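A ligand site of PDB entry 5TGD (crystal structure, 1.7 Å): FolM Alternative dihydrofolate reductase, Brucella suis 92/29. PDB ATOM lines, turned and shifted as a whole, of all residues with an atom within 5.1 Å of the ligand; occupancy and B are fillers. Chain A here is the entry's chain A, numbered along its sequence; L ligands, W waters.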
ATOM      1  N   GLY A  27     -27.466  13.841  -4.188  1.00  0.00           N
ATOM      2  CA  GLY A  27     -28.662  13.034  -4.287  1.00  0.00           C
ATOM      3  C   GLY A  27     -29.909  13.872  -4.082  1.00  0.00           C
ATOM      4  O   GLY A  27     -30.801  13.481  -3.331  1.00  0.00           O
ATOM      5  N   ALA A  29     -32.363  14.858  -6.177  1.00  0.00           N
ATOM      6  CA  ALA A  29     -33.456  14.817  -7.141  1.00  0.00           C
ATOM      7  C   ALA A  29     -34.687  14.047  -6.667  1.00  0.00           C
ATOM      8  O   ALA A  29     -35.704  14.072  -7.364  1.00  0.00           O
ATOM      9  CB  ALA A  29     -32.962  14.202  -8.463  1.00  0.00           C
ATOM     10  N   ARG A  30     -34.635  13.356  -5.533  1.00  0.00           N
ATOM     11  CA  ARG A  30     -35.800  12.613  -5.063  1.00  0.00           C
ATOM     12  C   ARG A  30     -35.903  12.699  -3.545  1.00  0.00           C
ATOM     13  O   ARG A  30     -34.943  13.071  -2.857  1.00  0.00           O
ATOM     14  CB  ARG A  30     -35.744  11.140  -5.483  1.00  0.00           C
ATOM     15  CG  ARG A  30     -35.328  10.930  -6.931  1.00  0.00           C
ATOM     16  CD  ARG A  30     -35.591   9.534  -7.421  1.00  0.00           C
ATOM     17  NE  ARG A  30     -37.005   9.192  -7.432  1.00  0.00           N
ATOM     18  CZ  ARG A  30     -37.515   8.085  -6.875  1.00  0.00           C
ATOM     19  NH1 ARG A  30     -36.717   7.214  -6.275  1.00  0.00           N
ATOM     20  NH2 ARG A  30     -38.819   7.862  -6.924  1.00  0.00           N
ATOM     21  N   ARG A  31     -37.088  12.359  -3.036  1.00  0.00           N
ATOM     22  CA  ARG A  31     -37.328  12.023  -1.620  1.00  0.00           C
ATOM     23  C   ARG A  31     -36.796  13.138  -0.718  1.00  0.00           C
ATOM     24  O   ARG A  31     -37.133  14.305  -0.946  1.00  0.00           O
ATOM     25  CB  ARG A  31     -36.746  10.627  -1.364  1.00  0.00           C
ATOM     26  CG  ARG A  31     -37.557   9.508  -2.003  1.00  0.00           C
ATOM     27  CD  ARG A  31     -36.798   8.178  -2.078  1.00  0.00           C
ATOM     28  NE  ARG A  31     -36.492   7.635  -0.755  1.00  0.00           N
ATOM     29  CZ  ARG A  31     -37.271   6.802  -0.067  1.00  0.00           C
ATOM     30  NH1 ARG A  31     -38.423   6.394  -0.579  1.00  0.00           N
ATOM     31  NH2 ARG A  31     -36.899   6.377   1.135  1.00  0.00           N
ATOM     32  N   ILE A  32     -35.987  12.838   0.310  1.00  0.00           N
ATOM     33  CA  ILE A  32     -35.572  13.854   1.272  1.00  0.00           C
ATOM     34  C   ILE A  32     -34.682  14.898   0.607  1.00  0.00           C
ATOM     35  O   ILE A  32     -34.803  16.095   0.873  1.00  0.00           O
ATOM     36  CB  ILE A  32     -34.864  13.187   2.460  1.00  0.00           C
ATOM     37  CG1 ILE A  32     -35.852  12.295   3.233  1.00  0.00           C
ATOM     38  CG2 ILE A  32     -34.240  14.238   3.357  1.00  0.00           C
ATOM     39  CD1 ILE A  32     -35.190  11.405   4.296  1.00  0.00           C
ATOM     40  N   GLY A  33     -33.764  14.448  -0.262  1.00  0.00           N
ATOM     41  CA  GLY A  33     -32.924  15.400  -0.980  1.00  0.00           C
ATOM     42  C   GLY A  33     -33.742  16.418  -1.737  1.00  0.00           C
ATOM     43  O   GLY A  33     -33.459  17.616  -1.677  1.00  0.00           O
ATOM     44  N   HIS A  50     -27.510  17.889  -7.255  1.00  0.00           N
ATOM     45  CA  HIS A  50     -26.699  16.792  -7.719  1.00  0.00           C
ATOM     46  C   HIS A  50     -27.542  15.526  -7.863  1.00  0.00           C
ATOM     47  O   HIS A  50     -28.414  15.248  -7.040  1.00  0.00           O
ATOM     48  CB  HIS A  50     -25.529  16.527  -6.783  1.00  0.00           C
ATOM     49  CG  HIS A  50     -24.938  15.176  -6.994  1.00  0.00           C
ATOM     50  ND1 HIS A  50     -25.378  14.068  -6.294  1.00  0.00           N
ATOM     51  CD2 HIS A  50     -24.033  14.718  -7.894  1.00  0.00           C
ATOM     52  CE1 HIS A  50     -24.738  12.999  -6.723  1.00  0.00           C
ATOM     53  NE2 HIS A  50     -23.921  13.366  -7.700  1.00  0.00           N
ATOM     54  N   CYS A  51     -27.256  14.757  -8.898  1.00  0.00           N
ATOM     55  CA  CYS A  51     -27.903  13.473  -9.109  1.00  0.00           C
ATOM     56  C   CYS A  51     -26.998  12.603  -9.972  1.00  0.00           C
ATOM     57  O   CYS A  51     -25.953  13.043 -10.478  1.00  0.00           O
ATOM     58  CB  CYS A  51     -29.289  13.646  -9.736  1.00  0.00           C
ATOM     59  SG  CYS A  51     -29.308  14.541 -11.307  1.00  0.00           S
ATOM     60  N   ASN A  52     -27.388  11.337 -10.124  1.00  0.00           N
ATOM     61  CA  ASN A  52     -26.693  10.402 -10.997  1.00  0.00           C
ATOM     62  C   ASN A  52     -27.701   9.679 -11.861  1.00  0.00           C
ATOM     63  O   ASN A  52     -27.820   9.960 -13.058  1.00  0.00           O
ATOM     64  CB  ASN A  52     -25.847   9.401 -10.192  1.00  0.00           C
ATOM     65  N   ARG A  53     -28.470   8.764 -11.260  1.00  0.00           N
ATOM     66  CA  ARG A  53     -29.500   8.065 -12.031  1.00  0.00           C
ATOM     67  C   ARG A  53     -30.702   8.972 -12.299  1.00  0.00           C
ATOM     68  O   ARG A  53     -31.285   8.915 -13.387  1.00  0.00           O
ATOM     69  CB  ARG A  53     -29.919   6.790 -11.298  1.00  0.00           C
ATOM     70  N   SER A  54     -31.057   9.852 -11.359  1.00  0.00           N
ATOM     71  CA  SER A  54     -32.315  10.583 -11.418  1.00  0.00           C
ATOM     72  C   SER A  54     -32.196  11.928 -12.161  1.00  0.00           C
ATOM     73  O   SER A  54     -32.700  12.951 -11.707  1.00  0.00           O
ATOM     74  CB  SER A  54     -32.855  10.787 -10.006  1.00  0.00           C
ATOM     75  OG  SER A  54     -33.057   9.545  -9.374  1.00  0.00           O
ATOM     76  N   LEU A  55     -31.543  11.918 -13.315  1.00  0.00           N
ATOM     77  CA  LEU A  55     -31.298  13.159 -14.042  1.00  0.00           C
ATOM     78  C   LEU A  55     -32.600  13.786 -14.527  1.00  0.00           C
ATOM     79  O   LEU A  55     -32.782  15.008 -14.415  1.00  0.00           O
ATOM     80  CB  LEU A  55     -30.358  12.891 -15.217  1.00  0.00           C
ATOM     81  CG  LEU A  55     -29.988  14.096 -16.085  1.00  0.00           C
ATOM     82  CD1 LEU A  55     -29.235  15.127 -15.284  1.00  0.00           C
ATOM     83  CD2 LEU A  55     -29.165  13.638 -17.260  1.00  0.00           C
ATOM     84  N   ALA A  77     -22.887  13.430 -11.238  1.00  0.00           N
ATOM     85  CA  ALA A  77     -21.619  12.780 -10.940  1.00  0.00           C
ATOM     86  C   ALA A  77     -21.888  11.479 -10.201  1.00  0.00           C
ATOM     87  O   ALA A  77     -22.856  11.362  -9.440  1.00  0.00           O
ATOM     88  CB  ALA A  77     -20.696  13.678 -10.114  1.00  0.00           C
ATOM     89  N   ASP A  78     -21.000  10.510 -10.426  1.00  0.00           N
ATOM     90  CA  ASP A  78     -21.010   9.273  -9.672  1.00  0.00           C
ATOM     91  C   ASP A  78     -20.216   9.506  -8.389  1.00  0.00           C
ATOM     92  O   ASP A  78     -19.005   9.731  -8.443  1.00  0.00           O
ATOM     93  CB  ASP A  78     -20.390   8.148 -10.505  1.00  0.00           C
ATOM     94  CG  ASP A  78     -20.458   6.781  -9.823  1.00  0.00           C
ATOM     95  OD1 ASP A  78     -20.606   6.702  -8.581  1.00  0.00           O
ATOM     96  OD2 ASP A  78     -20.331   5.780 -10.552  1.00  0.00           O
ATOM     97  N   LEU A  79     -20.903   9.459  -7.245  1.00  0.00           N
ATOM     98  CA  LEU A  79     -20.192   9.697  -5.992  1.00  0.00           C
ATOM     99  C   LEU A  79     -19.285   8.533  -5.572  1.00  0.00           C
ATOM    100  O   LEU A  79     -18.607   8.648  -4.545  1.00  0.00           O
ATOM    101  CB  LEU A  79     -21.193  10.021  -4.882  1.00  0.00           C
ATOM    102  CG  LEU A  79     -22.025  11.281  -5.139  1.00  0.00           C
ATOM    103  CD1 LEU A  79     -22.895  11.621  -3.940  1.00  0.00           C
ATOM    104  CD2 LEU A  79     -21.152  12.462  -5.495  1.00  0.00           C
ATOM    105  N   GLU A  80     -19.233   7.430  -6.322  1.00  0.00           N
ATOM    106  CA  GLU A  80     -18.252   6.400  -6.057  1.00  0.00           C
ATOM    107  C   GLU A  80     -17.105   6.426  -7.052  1.00  0.00           C
ATOM    108  O   GLU A  80     -16.209   5.561  -6.984  1.00  0.00           O
ATOM    109  CB  GLU A  80     -18.912   5.020  -6.058  1.00  0.00           C
ATOM    110  CG  GLU A  80     -20.061   4.933  -5.092  1.00  0.00           C
ATOM    111  CD  GLU A  80     -20.815   3.641  -5.230  1.00  0.00           C
ATOM    112  OE1 GLU A  80     -20.176   2.575  -5.151  1.00  0.00           O
ATOM    113  OE2 GLU A  80     -22.050   3.684  -5.419  1.00  0.00           O
ATOM    114  N   ASN A 102     -24.661  16.869   2.416  1.00  0.00           N
ATOM    115  CA  ASN A 102     -24.234  15.515   2.058  1.00  0.00           C
ATOM    116  C   ASN A 102     -25.403  14.583   2.326  1.00  0.00           C
ATOM    117  O   ASN A 102     -25.535  14.000   3.402  1.00  0.00           O
ATOM    118  CB  ASN A 102     -22.985  15.123   2.830  1.00  0.00           C
ATOM    119  CG  ASN A 102     -21.742  15.744   2.246  1.00  0.00           C
ATOM    120  OD1 ASN A 102     -21.510  15.690   1.026  1.00  0.00           O
ATOM    121  ND2 ASN A 102     -20.933  16.365   3.105  1.00  0.00           N
ATOM    122  N   ASN A 103     -26.269  14.450   1.326  1.00  0.00           N
ATOM    123  CA  ASN A 103     -27.507  13.706   1.487  1.00  0.00           C
ATOM    124  C   ASN A 103     -27.463  12.338   0.820  1.00  0.00           C
ATOM    125  O   ASN A 103     -28.117  11.410   1.310  1.00  0.00           O
ATOM    126  CB  ASN A 103     -28.671  14.533   0.913  1.00  0.00           C
ATOM    127  CG  ASN A 103     -29.965  13.744   0.819  1.00  0.00           C
ATOM    128  OD1 ASN A 103     -30.626  13.499   1.827  1.00  0.00           O
ATOM    129  ND2 ASN A 103     -30.335  13.333  -0.396  1.00  0.00           N
ATOM    130  N   ALA A 104     -26.709  12.196  -0.274  1.00  0.00           N
ATOM    131  CA  ALA A 104     -26.714  10.944  -1.026  1.00  0.00           C
ATOM    132  C   ALA A 104     -26.338   9.749  -0.146  1.00  0.00           C
ATOM    133  O   ALA A 104     -25.571   9.859   0.819  1.00  0.00           O
ATOM    134  CB  ALA A 104     -25.733  11.045  -2.181  1.00  0.00           C
ATOM    135  N   SER A 105     -26.875   8.597  -0.501  1.00  0.00           N
ATOM    136  CA  SER A 105     -26.789   7.454   0.375  1.00  0.00           C
ATOM    137  C   SER A 105     -26.989   6.173  -0.402  1.00  0.00           C
ATOM    138  O   SER A 105     -27.605   6.162  -1.474  1.00  0.00           O
ATOM    139  CB  SER A 105     -27.825   7.556   1.491  1.00  0.00           C
ATOM    140  OG  SER A 105     -27.924   6.338   2.201  1.00  0.00           O
ATOM    141  N   LEU A 106     -26.482   5.089   0.170  1.00  0.00           N
ATOM    142  CA  LEU A 106     -26.792   3.733  -0.213  1.00  0.00           C
ATOM    143  C   LEU A 106     -27.176   2.996   1.068  1.00  0.00           C
ATOM    144  O   LEU A 106     -26.546   3.199   2.100  1.00  0.00           O
ATOM    145  CB  LEU A 106     -25.595   3.071  -0.905  1.00  0.00           C
ATOM    146  CG  LEU A 106     -25.658   1.611  -1.330  1.00  0.00           C
ATOM    147  CD1 LEU A 106     -26.705   1.410  -2.415  1.00  0.00           C
ATOM    148  CD2 LEU A 106     -24.276   1.176  -1.809  1.00  0.00           C
ATOM    149  N   ARG A 122     -18.614   0.368  -0.735  1.00  0.00           N
ATOM    150  CA  ARG A 122     -19.552   1.314  -1.313  1.00  0.00           C
ATOM    151  C   ARG A 122     -20.209   2.171  -0.238  1.00  0.00           C
ATOM    152  O   ARG A 122     -20.389   3.383  -0.421  1.00  0.00           O
ATOM    153  CB  ARG A 122     -20.630   0.584  -2.107  1.00  0.00           C
ATOM    154  CG  ARG A 122     -20.106  -0.276  -3.241  1.00  0.00           C
ATOM    155  CD  ARG A 122     -21.240  -0.671  -4.151  1.00  0.00           C
ATOM    156  NE  ARG A 122     -21.770   0.473  -4.876  1.00  0.00           N
ATOM    157  CZ  ARG A 122     -22.919   0.467  -5.541  1.00  0.00           C
ATOM    158  NH1 ARG A 122     -23.677  -0.620  -5.547  1.00  0.00           N
ATOM    159  NH2 ARG A 122     -23.327   1.552  -6.187  1.00  0.00           N
ATOM    160  N   VAL A 126     -19.776   6.353  -0.199  1.00  0.00           N
ATOM    161  CA  VAL A 126     -20.866   7.314  -0.348  1.00  0.00           C
ATOM    162  C   VAL A 126     -21.098   8.090   0.952  1.00  0.00           C
ATOM    163  O   VAL A 126     -21.418   9.286   0.923  1.00  0.00           O
ATOM    164  CB  VAL A 126     -22.152   6.599  -0.805  1.00  0.00           C
ATOM    165  CG1 VAL A 126     -23.316   7.556  -0.876  1.00  0.00           C
ATOM    166  CG2 VAL A 126     -21.936   5.917  -2.166  1.00  0.00           C
ATOM    167  N   HIS A 127     -20.943   7.443   2.095  1.00  0.00           N
ATOM    168  CA  HIS A 127     -21.302   8.093   3.358  1.00  0.00           C
ATOM    169  C   HIS A 127     -20.135   8.750   4.067  1.00  0.00           C
ATOM    170  O   HIS A 127     -20.361   9.584   4.944  1.00  0.00           O
ATOM    171  CB  HIS A 127     -21.951   7.097   4.314  1.00  0.00           C
ATOM    172  CG  HIS A 127     -23.162   6.429   3.749  1.00  0.00           C
ATOM    173  ND1 HIS A 127     -23.496   5.129   4.058  1.00  0.00           N
ATOM    174  CD2 HIS A 127     -24.105   6.880   2.889  1.00  0.00           C
ATOM    175  CE1 HIS A 127     -24.598   4.795   3.402  1.00  0.00           C
ATOM    176  NE2 HIS A 127     -24.980   5.842   2.690  1.00  0.00           N
ATOM    177  N   ILE A 153     -26.204  14.356   6.172  1.00  0.00           N
ATOM    178  CA  ILE A 153     -27.399  13.583   6.463  1.00  0.00           C
ATOM    179  C   ILE A 153     -26.966  12.183   6.874  1.00  0.00           C
ATOM    180  O   ILE A 153     -26.357  11.443   6.087  1.00  0.00           O
ATOM    181  CB  ILE A 153     -28.366  13.528   5.275  1.00  0.00           C
ATOM    182  CG1 ILE A 153     -28.583  14.928   4.688  1.00  0.00           C
ATOM    183  CG2 ILE A 153     -29.681  12.990   5.753  1.00  0.00           C
ATOM    184  CD1 ILE A 153     -29.115  15.959   5.712  1.00  0.00           C
ATOM    185  N   ILE A 154     -27.282  11.811   8.113  1.00  0.00           N
ATOM    186  CA  ILE A 154     -26.760  10.568   8.653  1.00  0.00           C
ATOM    187  C   ILE A 154     -27.928   9.605   8.831  1.00  0.00           C
ATOM    188  O   ILE A 154     -28.551   9.201   7.833  1.00  0.00           O
ATOM    189  CB  ILE A 154     -25.983  10.840   9.953  1.00  0.00           C
ATOM    190  CG1 ILE A 154     -25.121  12.101   9.755  1.00  0.00           C
ATOM    191  CG2 ILE A 154     -25.132   9.621  10.346  1.00  0.00           C
ATOM    192  CD1 ILE A 154     -24.032  12.315  10.775  1.00  0.00           C
ATOM    193  N   ASP A 155     -28.227   9.244  10.073  1.00  0.00           N
ATOM    194  CA  ASP A 155     -29.238   8.229  10.377  1.00  0.00           C
ATOM    195  C   ASP A 155     -29.336   8.180  11.894  1.00  0.00           C
ATOM    196  O   ASP A 155     -28.308   8.181  12.566  1.00  0.00           O
ATOM    197  CB  ASP A 155     -28.828   6.865   9.823  1.00  0.00           C
ATOM    198  CG  ASP A 155     -29.919   5.793   9.975  1.00  0.00           C
ATOM    199  OD1 ASP A 155     -30.587   5.747  11.021  1.00  0.00           O
ATOM    200  OD2 ASP A 155     -30.084   4.979   9.036  1.00  0.00           O
ATOM    201  N   TYR A 168     -23.388  -0.691   6.613  1.00  0.00           N
ATOM    202  CA  TYR A 168     -24.116   0.573   6.504  1.00  0.00           C
ATOM    203  C   TYR A 168     -24.015   1.361   7.806  1.00  0.00           C
ATOM    204  O   TYR A 168     -23.684   2.561   7.800  1.00  0.00           O
ATOM    205  CB  TYR A 168     -25.581   0.313   6.154  1.00  0.00           C
ATOM    206  CG  TYR A 168     -26.465   1.529   6.265  1.00  0.00           C
ATOM    207  CD1 TYR A 168     -26.570   2.436   5.223  1.00  0.00           C
ATOM    208  CD2 TYR A 168     -27.194   1.778   7.425  1.00  0.00           C
ATOM    209  CE1 TYR A 168     -27.383   3.565   5.333  1.00  0.00           C
ATOM    210  CE2 TYR A 168     -28.001   2.910   7.550  1.00  0.00           C
ATOM    211  CZ  TYR A 168     -28.096   3.790   6.491  1.00  0.00           C
ATOM    212  OH  TYR A 168     -28.903   4.905   6.614  1.00  0.00           O
ATOM    213  N   LYS A 172     -22.276   5.103   8.424  1.00  0.00           N
ATOM    214  CA  LYS A 172     -23.016   6.263   8.932  1.00  0.00           C
ATOM    215  C   LYS A 172     -22.465   6.714  10.279  1.00  0.00           C
ATOM    216  O   LYS A 172     -22.369   7.913  10.547  1.00  0.00           O
ATOM    217  CB  LYS A 172     -24.503   5.943   9.037  1.00  0.00           C
ATOM    218  CG  LYS A 172     -25.227   5.836   7.712  1.00  0.00           C
ATOM    219  CD  LYS A 172     -25.473   7.218   7.091  1.00  0.00           C
ATOM    220  CE  LYS A 172     -26.507   7.114   5.975  1.00  0.00           C
ATOM    221  NZ  LYS A 172     -26.939   8.444   5.420  1.00  0.00           N
ATOM    222  N   PRO A 197     -32.037  11.339  10.232  1.00  0.00           N
ATOM    223  CA  PRO A 197     -33.449  10.998  10.013  1.00  0.00           C
ATOM    224  C   PRO A 197     -33.820   9.691  10.676  1.00  0.00           C
ATOM    225  O   PRO A 197     -33.013   8.756  10.747  1.00  0.00           O
ATOM    226  CB  PRO A 197     -33.567  10.901   8.484  1.00  0.00           C
ATOM    227  CG  PRO A 197     -32.323  11.563   7.941  1.00  0.00           C
ATOM    228  CD  PRO A 197     -31.262  11.338   8.985  1.00  0.00           C
ATOM    229  N   GLY A 198     -35.046   9.633  11.171  1.00  0.00           N
ATOM    230  CA  GLY A 198     -35.687   8.372  11.487  1.00  0.00           C
ATOM    231  C   GLY A 198     -36.586   7.967  10.336  1.00  0.00           C
ATOM    232  O   GLY A 198     -36.404   8.406   9.183  1.00  0.00           O
ATOM    233  N   PRO A 199     -37.592   7.135  10.612  1.00  0.00           N
ATOM    234  CA  PRO A 199     -38.475   6.670   9.528  1.00  0.00           C
ATOM    235  C   PRO A 199     -39.232   7.818   8.886  1.00  0.00           C
ATOM    236  O   PRO A 199     -40.180   8.382   9.451  1.00  0.00           O
ATOM    237  CB  PRO A 199     -39.414   5.685  10.245  1.00  0.00           C
ATOM    238  CG  PRO A 199     -38.676   5.308  11.528  1.00  0.00           C
ATOM    239  CD  PRO A 199     -37.974   6.570  11.914  1.00  0.00           C
ATOM    240  N   THR A 200     -38.797   8.201   7.691  1.00  0.00           N
ATOM    241  CA  THR A 200     -39.350   9.354   6.986  1.00  0.00           C
ATOM    242  C   THR A 200     -40.132   8.946   5.748  1.00  0.00           C
ATOM    243  O   THR A 200     -41.251   9.419   5.545  1.00  0.00           O
ATOM    244  CB  THR A 200     -38.225  10.313   6.602  1.00  0.00           C
ATOM    245  OG1 THR A 200     -37.408  10.585   7.750  1.00  0.00           O
ATOM    246  CG2 THR A 200     -38.799  11.615   6.057  1.00  0.00           C
ATOM    247  N   LEU A 201     -39.564   8.077   4.926  1.00  0.00           N
ATOM    248  CA  LEU A 201     -40.243   7.549   3.756  1.00  0.00           C
ATOM    249  C   LEU A 201     -39.882   6.077   3.713  1.00  0.00           C
ATOM    250  O   LEU A 201     -38.687   5.744   3.856  1.00  0.00           O
ATOM    251  CB  LEU A 201     -39.833   8.252   2.460  1.00  0.00           C
ATOM    252  CG  LEU A 201     -40.212   9.735   2.373  1.00  0.00           C
ATOM    253  CD1 LEU A 201     -39.524  10.375   1.179  1.00  0.00           C
ATOM    254  CD2 LEU A 201     -41.724   9.901   2.305  1.00  0.00           C
HETATM  255  P1  LIG L   1     -32.130   7.689  -1.197  1.00  0.00           P
HETATM  256  O1  LIG L   1     -33.377   7.996  -1.936  1.00  0.00           O
HETATM  257  O2  LIG L   1     -32.054   6.196  -0.887  1.00  0.00           O
HETATM  258  O3  LIG L   1     -30.785   8.038  -1.996  1.00  0.00           O
HETATM  259  C1  LIG L   1     -30.316   9.386  -2.098  1.00  0.00           C
HETATM  260  C2  LIG L   1     -29.626   9.555  -3.434  1.00  0.00           C
HETATM  261  O4  LIG L   1     -28.234   9.213  -3.336  1.00  0.00           O
HETATM  262  C3  LIG L   1     -30.123   8.696  -4.588  1.00  0.00           C
HETATM  263  O5  LIG L   1     -31.277   9.233  -5.217  1.00  0.00           O
HETATM  264  C4  LIG L   1     -28.929   8.822  -5.537  1.00  0.00           C
HETATM  265  O6  LIG L   1     -29.125   9.820  -6.550  1.00  0.00           O
HETATM  266  C5  LIG L   1     -27.753   9.256  -4.667  1.00  0.00           C
HETATM  267  N1  LIG L   1     -26.576   8.410  -4.803  1.00  0.00           N
HETATM  268  C6  LIG L   1     -26.332   7.190  -4.227  1.00  0.00           C
HETATM  269  N2  LIG L   1     -25.224   6.618  -4.638  1.00  0.00           N
HETATM  270  C7  LIG L   1     -24.690   7.534  -5.544  1.00  0.00           C
HETATM  271  C8  LIG L   1     -23.529   7.518  -6.335  1.00  0.00           C
HETATM  272  N3  LIG L   1     -22.656   6.513  -6.365  1.00  0.00           N
HETATM  273  N4  LIG L   1     -23.298   8.599  -7.126  1.00  0.00           N
HETATM  274  C9  LIG L   1     -24.186   9.596  -7.126  1.00  0.00           C
HETATM  275  N5  LIG L   1     -25.309   9.709  -6.420  1.00  0.00           N
HETATM  276  C10 LIG L   1     -25.510   8.641  -5.646  1.00  0.00           C
HETATM  277  O7  LIG L   1     -32.132   8.481   0.187  1.00  0.00           O
HETATM  278  P2  LIG L   1     -33.370   8.987   1.070  1.00  0.00           P
HETATM  279  O8  LIG L   1     -34.215   7.833   1.441  1.00  0.00           O
HETATM  280  O9  LIG L   1     -33.999  10.178   0.441  1.00  0.00           O
HETATM  281  O10 LIG L   1     -32.652   9.483   2.398  1.00  0.00           O
HETATM  282  C11 LIG L   1     -31.900  10.712   2.384  1.00  0.00           C
HETATM  283  C12 LIG L   1     -30.888  10.614   3.488  1.00  0.00           C
HETATM  284  O11 LIG L   1     -31.558  10.285   4.714  1.00  0.00           O
HETATM  285  C13 LIG L   1     -29.820   9.535   3.276  1.00  0.00           C
HETATM  286  O12 LIG L   1     -28.506   9.966   3.631  1.00  0.00           O
HETATM  287  C14 LIG L   1     -30.334   8.371   4.119  1.00  0.00           C
HETATM  288  O13 LIG L   1     -29.287   7.530   4.586  1.00  0.00           O
HETATM  289  C15 LIG L   1     -31.002   9.115   5.266  1.00  0.00           C
HETATM  290  N6  LIG L   1     -32.104   8.329   5.946  1.00  0.00           N
HETATM  291  C16 LIG L   1     -33.305   8.277   5.334  1.00  0.00           C
HETATM  292  C17 LIG L   1     -34.380   7.699   5.970  1.00  0.00           C
HETATM  293  C18 LIG L   1     -35.710   7.528   5.301  1.00  0.00           C
HETATM  294  O14 LIG L   1     -36.696   7.222   5.986  1.00  0.00           O
HETATM  295  N7  LIG L   1     -35.805   7.804   3.998  1.00  0.00           N
HETATM  296  C19 LIG L   1     -34.191   7.147   7.236  1.00  0.00           C
HETATM  297  C20 LIG L   1     -32.938   7.184   7.823  1.00  0.00           C
HETATM  298  C21 LIG L   1     -31.893   7.778   7.157  1.00  0.00           C
HETATM  299  P3  LIG L   1     -29.579   9.338  -8.033  1.00  0.00           P
HETATM  300  O15 LIG L   1     -30.880   8.617  -7.819  1.00  0.00           O
HETATM  301  O16 LIG L   1     -29.712  10.627  -8.861  1.00  0.00           O
HETATM  302  O17 LIG L   1     -28.438   8.488  -8.603  1.00  0.00           O
HETATM  303  O   HOH W   1     -33.569   8.001  -4.400  1.00  0.00           O
HETATM  304  O   HOH W   2     -32.971  11.838  -1.002  1.00  0.00           O
HETATM  305  O   HOH W   3     -29.968   4.904  -2.881  1.00  0.00           O
HETATM  306  O   HOH W   4     -24.441   3.994  -4.256  1.00  0.00           O
HETATM  307  O   HOH W   5     -30.740  12.490  -6.817  1.00  0.00           O
HETATM  308  O   HOH W   6     -32.703  11.445  -4.229  1.00  0.00           O
HETATM  309  O   HOH W   7     -25.224  10.163   3.874  1.00  0.00           O
HETATM  310  O   HOH W   8     -32.537   5.559   2.415  1.00  0.00           O
HETATM  311  O   HOH W   9     -31.631   5.103   5.147  1.00  0.00           O
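O14 of the ligand lies close to O of Gly 198 (3.4 Å).
Merely in contact with the ligand: Gly 27 (3.7 Å), His 50 (3.4 Å), Cys 51 (3.2 Å), Ala 77 (3.2 Å), Ala 104 (3.3 Å), Ile 153 (3.5 Å), Ile 154 (3.6 Å), Asp 155 (3.8 Å), Pro 197 (3.3 Å) and Pro 199 (3.9 Å).
Hydrophobic or aromatic side chains that line the ligand: Ile 32, His 50, Leu 79, Ala 104, Ile 153 and Pro 197.
Of the 34 residues printed, 25 come within 4 Å of the ligand.
The nearest printed residue that does not touch the ligand is Val 126 (4.2 Å).
Water W4 lies within hydrogen-bond range of the side-chain carboxylate (OE2) of Glu 80, a nitrogen (N2) of the ligand and the guanidinium group (NH2) of Arg 122.
Water W6 lies within hydrogen-bond range of O5 of the ligand, O of Gly 27 and N of Arg 30.
Water W5 bridges the backbone NH (N) of Ala 29 and an oxygen (O16) of the ligand.
Water W3 lies within hydrogen-bond range of the backbone carbonyl oxygen of Ser 105 (3.0 Å) and an oxygen (O2) of the ligand (3.2 Å).
Water W7 lies within hydrogen-bond range of O of Ile 153 (2.8 Å), NZ of Lys 172 (2.9 Å), O of Ala 104 (3.1 Å) and O12 of the ligand (3.3 Å).
Water W9 lies within hydrogen-bond range of OH of Tyr 168 (3.1 Å) and O13 of the ligand (3.4 Å).
O of Ile 153 lies within hydrogen-bond range of NZ of Lys 172 (3.1 Å).
The side-chain amino group (NZ) of Lys 172 lies within hydrogen-bond range of the backbone carbonyl oxygen (O) of Ile 154, 3.0 Å away.
O of Ser 54 sits at hydrogen-bond distance from SG of Cys 51, 3.8 Å away.
OG of Ser 105 lies within hydrogen-bond range of NE2 of His 127 (3.0 Å).
The backbone NH (N) of Glu 80 is in hydrogen-bond range of the side-chain carboxylate (OD1) of Asp 78 (2.7 Å).
The side-chain hydroxyl (OH) of Tyr 168 sits at hydrogen-bond distance from the side-chain carboxylate (OD2) of Asp 155 (2.7 Å).
ND1 of His 50 lies within hydrogen-bond range of N of Gly 27 (3.0 Å).
The backbone carbonyl oxygen of Asn 102 sits at hydrogen-bond distance from the backbone NH of Ile 153.
The backbone NH (N) of Leu 79 sits at hydrogen-bond distance from a nitrogen (N4) of the ligand, 2.5 Å away.
An oxygen (O13) of the ligand sits at hydrogen-bond distance from the side-chain amino group (NZ) of Lys 172 (2.7 Å).
O17 of the ligand sits at hydrogen-bond distance from N of Arg 53.
N of Asn 52 lies within hydrogen-bond range of O16 of the ligand (2.7 Å).
The backbone carbonyl oxygen of Asn 103 is in hydrogen-bond range of an oxygen (O12) of the ligand (2.8 Å).
The backbone NH (N) of Ser 54 is in hydrogen-bond range of an oxygen (O16) of the ligand (2.9 Å).
OG of Ser 54 lies within hydrogen-bond range of O15 of the ligand (2.8 Å).
O14 of the ligand lies within hydrogen-bond range of N of Thr 200 (2.9 Å).
The backbone NH of Ser 105 sits at hydrogen-bond distance from an oxygen (O4) of the ligand.
The side-chain hydroxyl of Ser 105 sits at hydrogen-bond distance from an oxygen (O13) of the ligand (3.0 Å).
The side-chain carboxylate of Asp 78 lies within hydrogen-bond range of a nitrogen (N3) of the ligand (3.0 Å).
The side-chain carboxylate (OE2) of Glu 80 sits at hydrogen-bond distance from a nitrogen (N3) of the ligand, at 3.0 Å.
An oxygen (O8) of the ligand lies within salt-bridge range of the guanidinium group of Arg 31 (3.1 Å).
The backbone NH of Leu 201 is in hydrogen-bond range of an oxygen (O14) of the ligand.
N of Ile 32 is in hydrogen-bond range of O9 of the ligand (3.3 Å).
An oxygen (O13) of the ligand lies within hydrogen-bond range of the side-chain hydroxyl of Tyr 168, at 3.3 Å.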
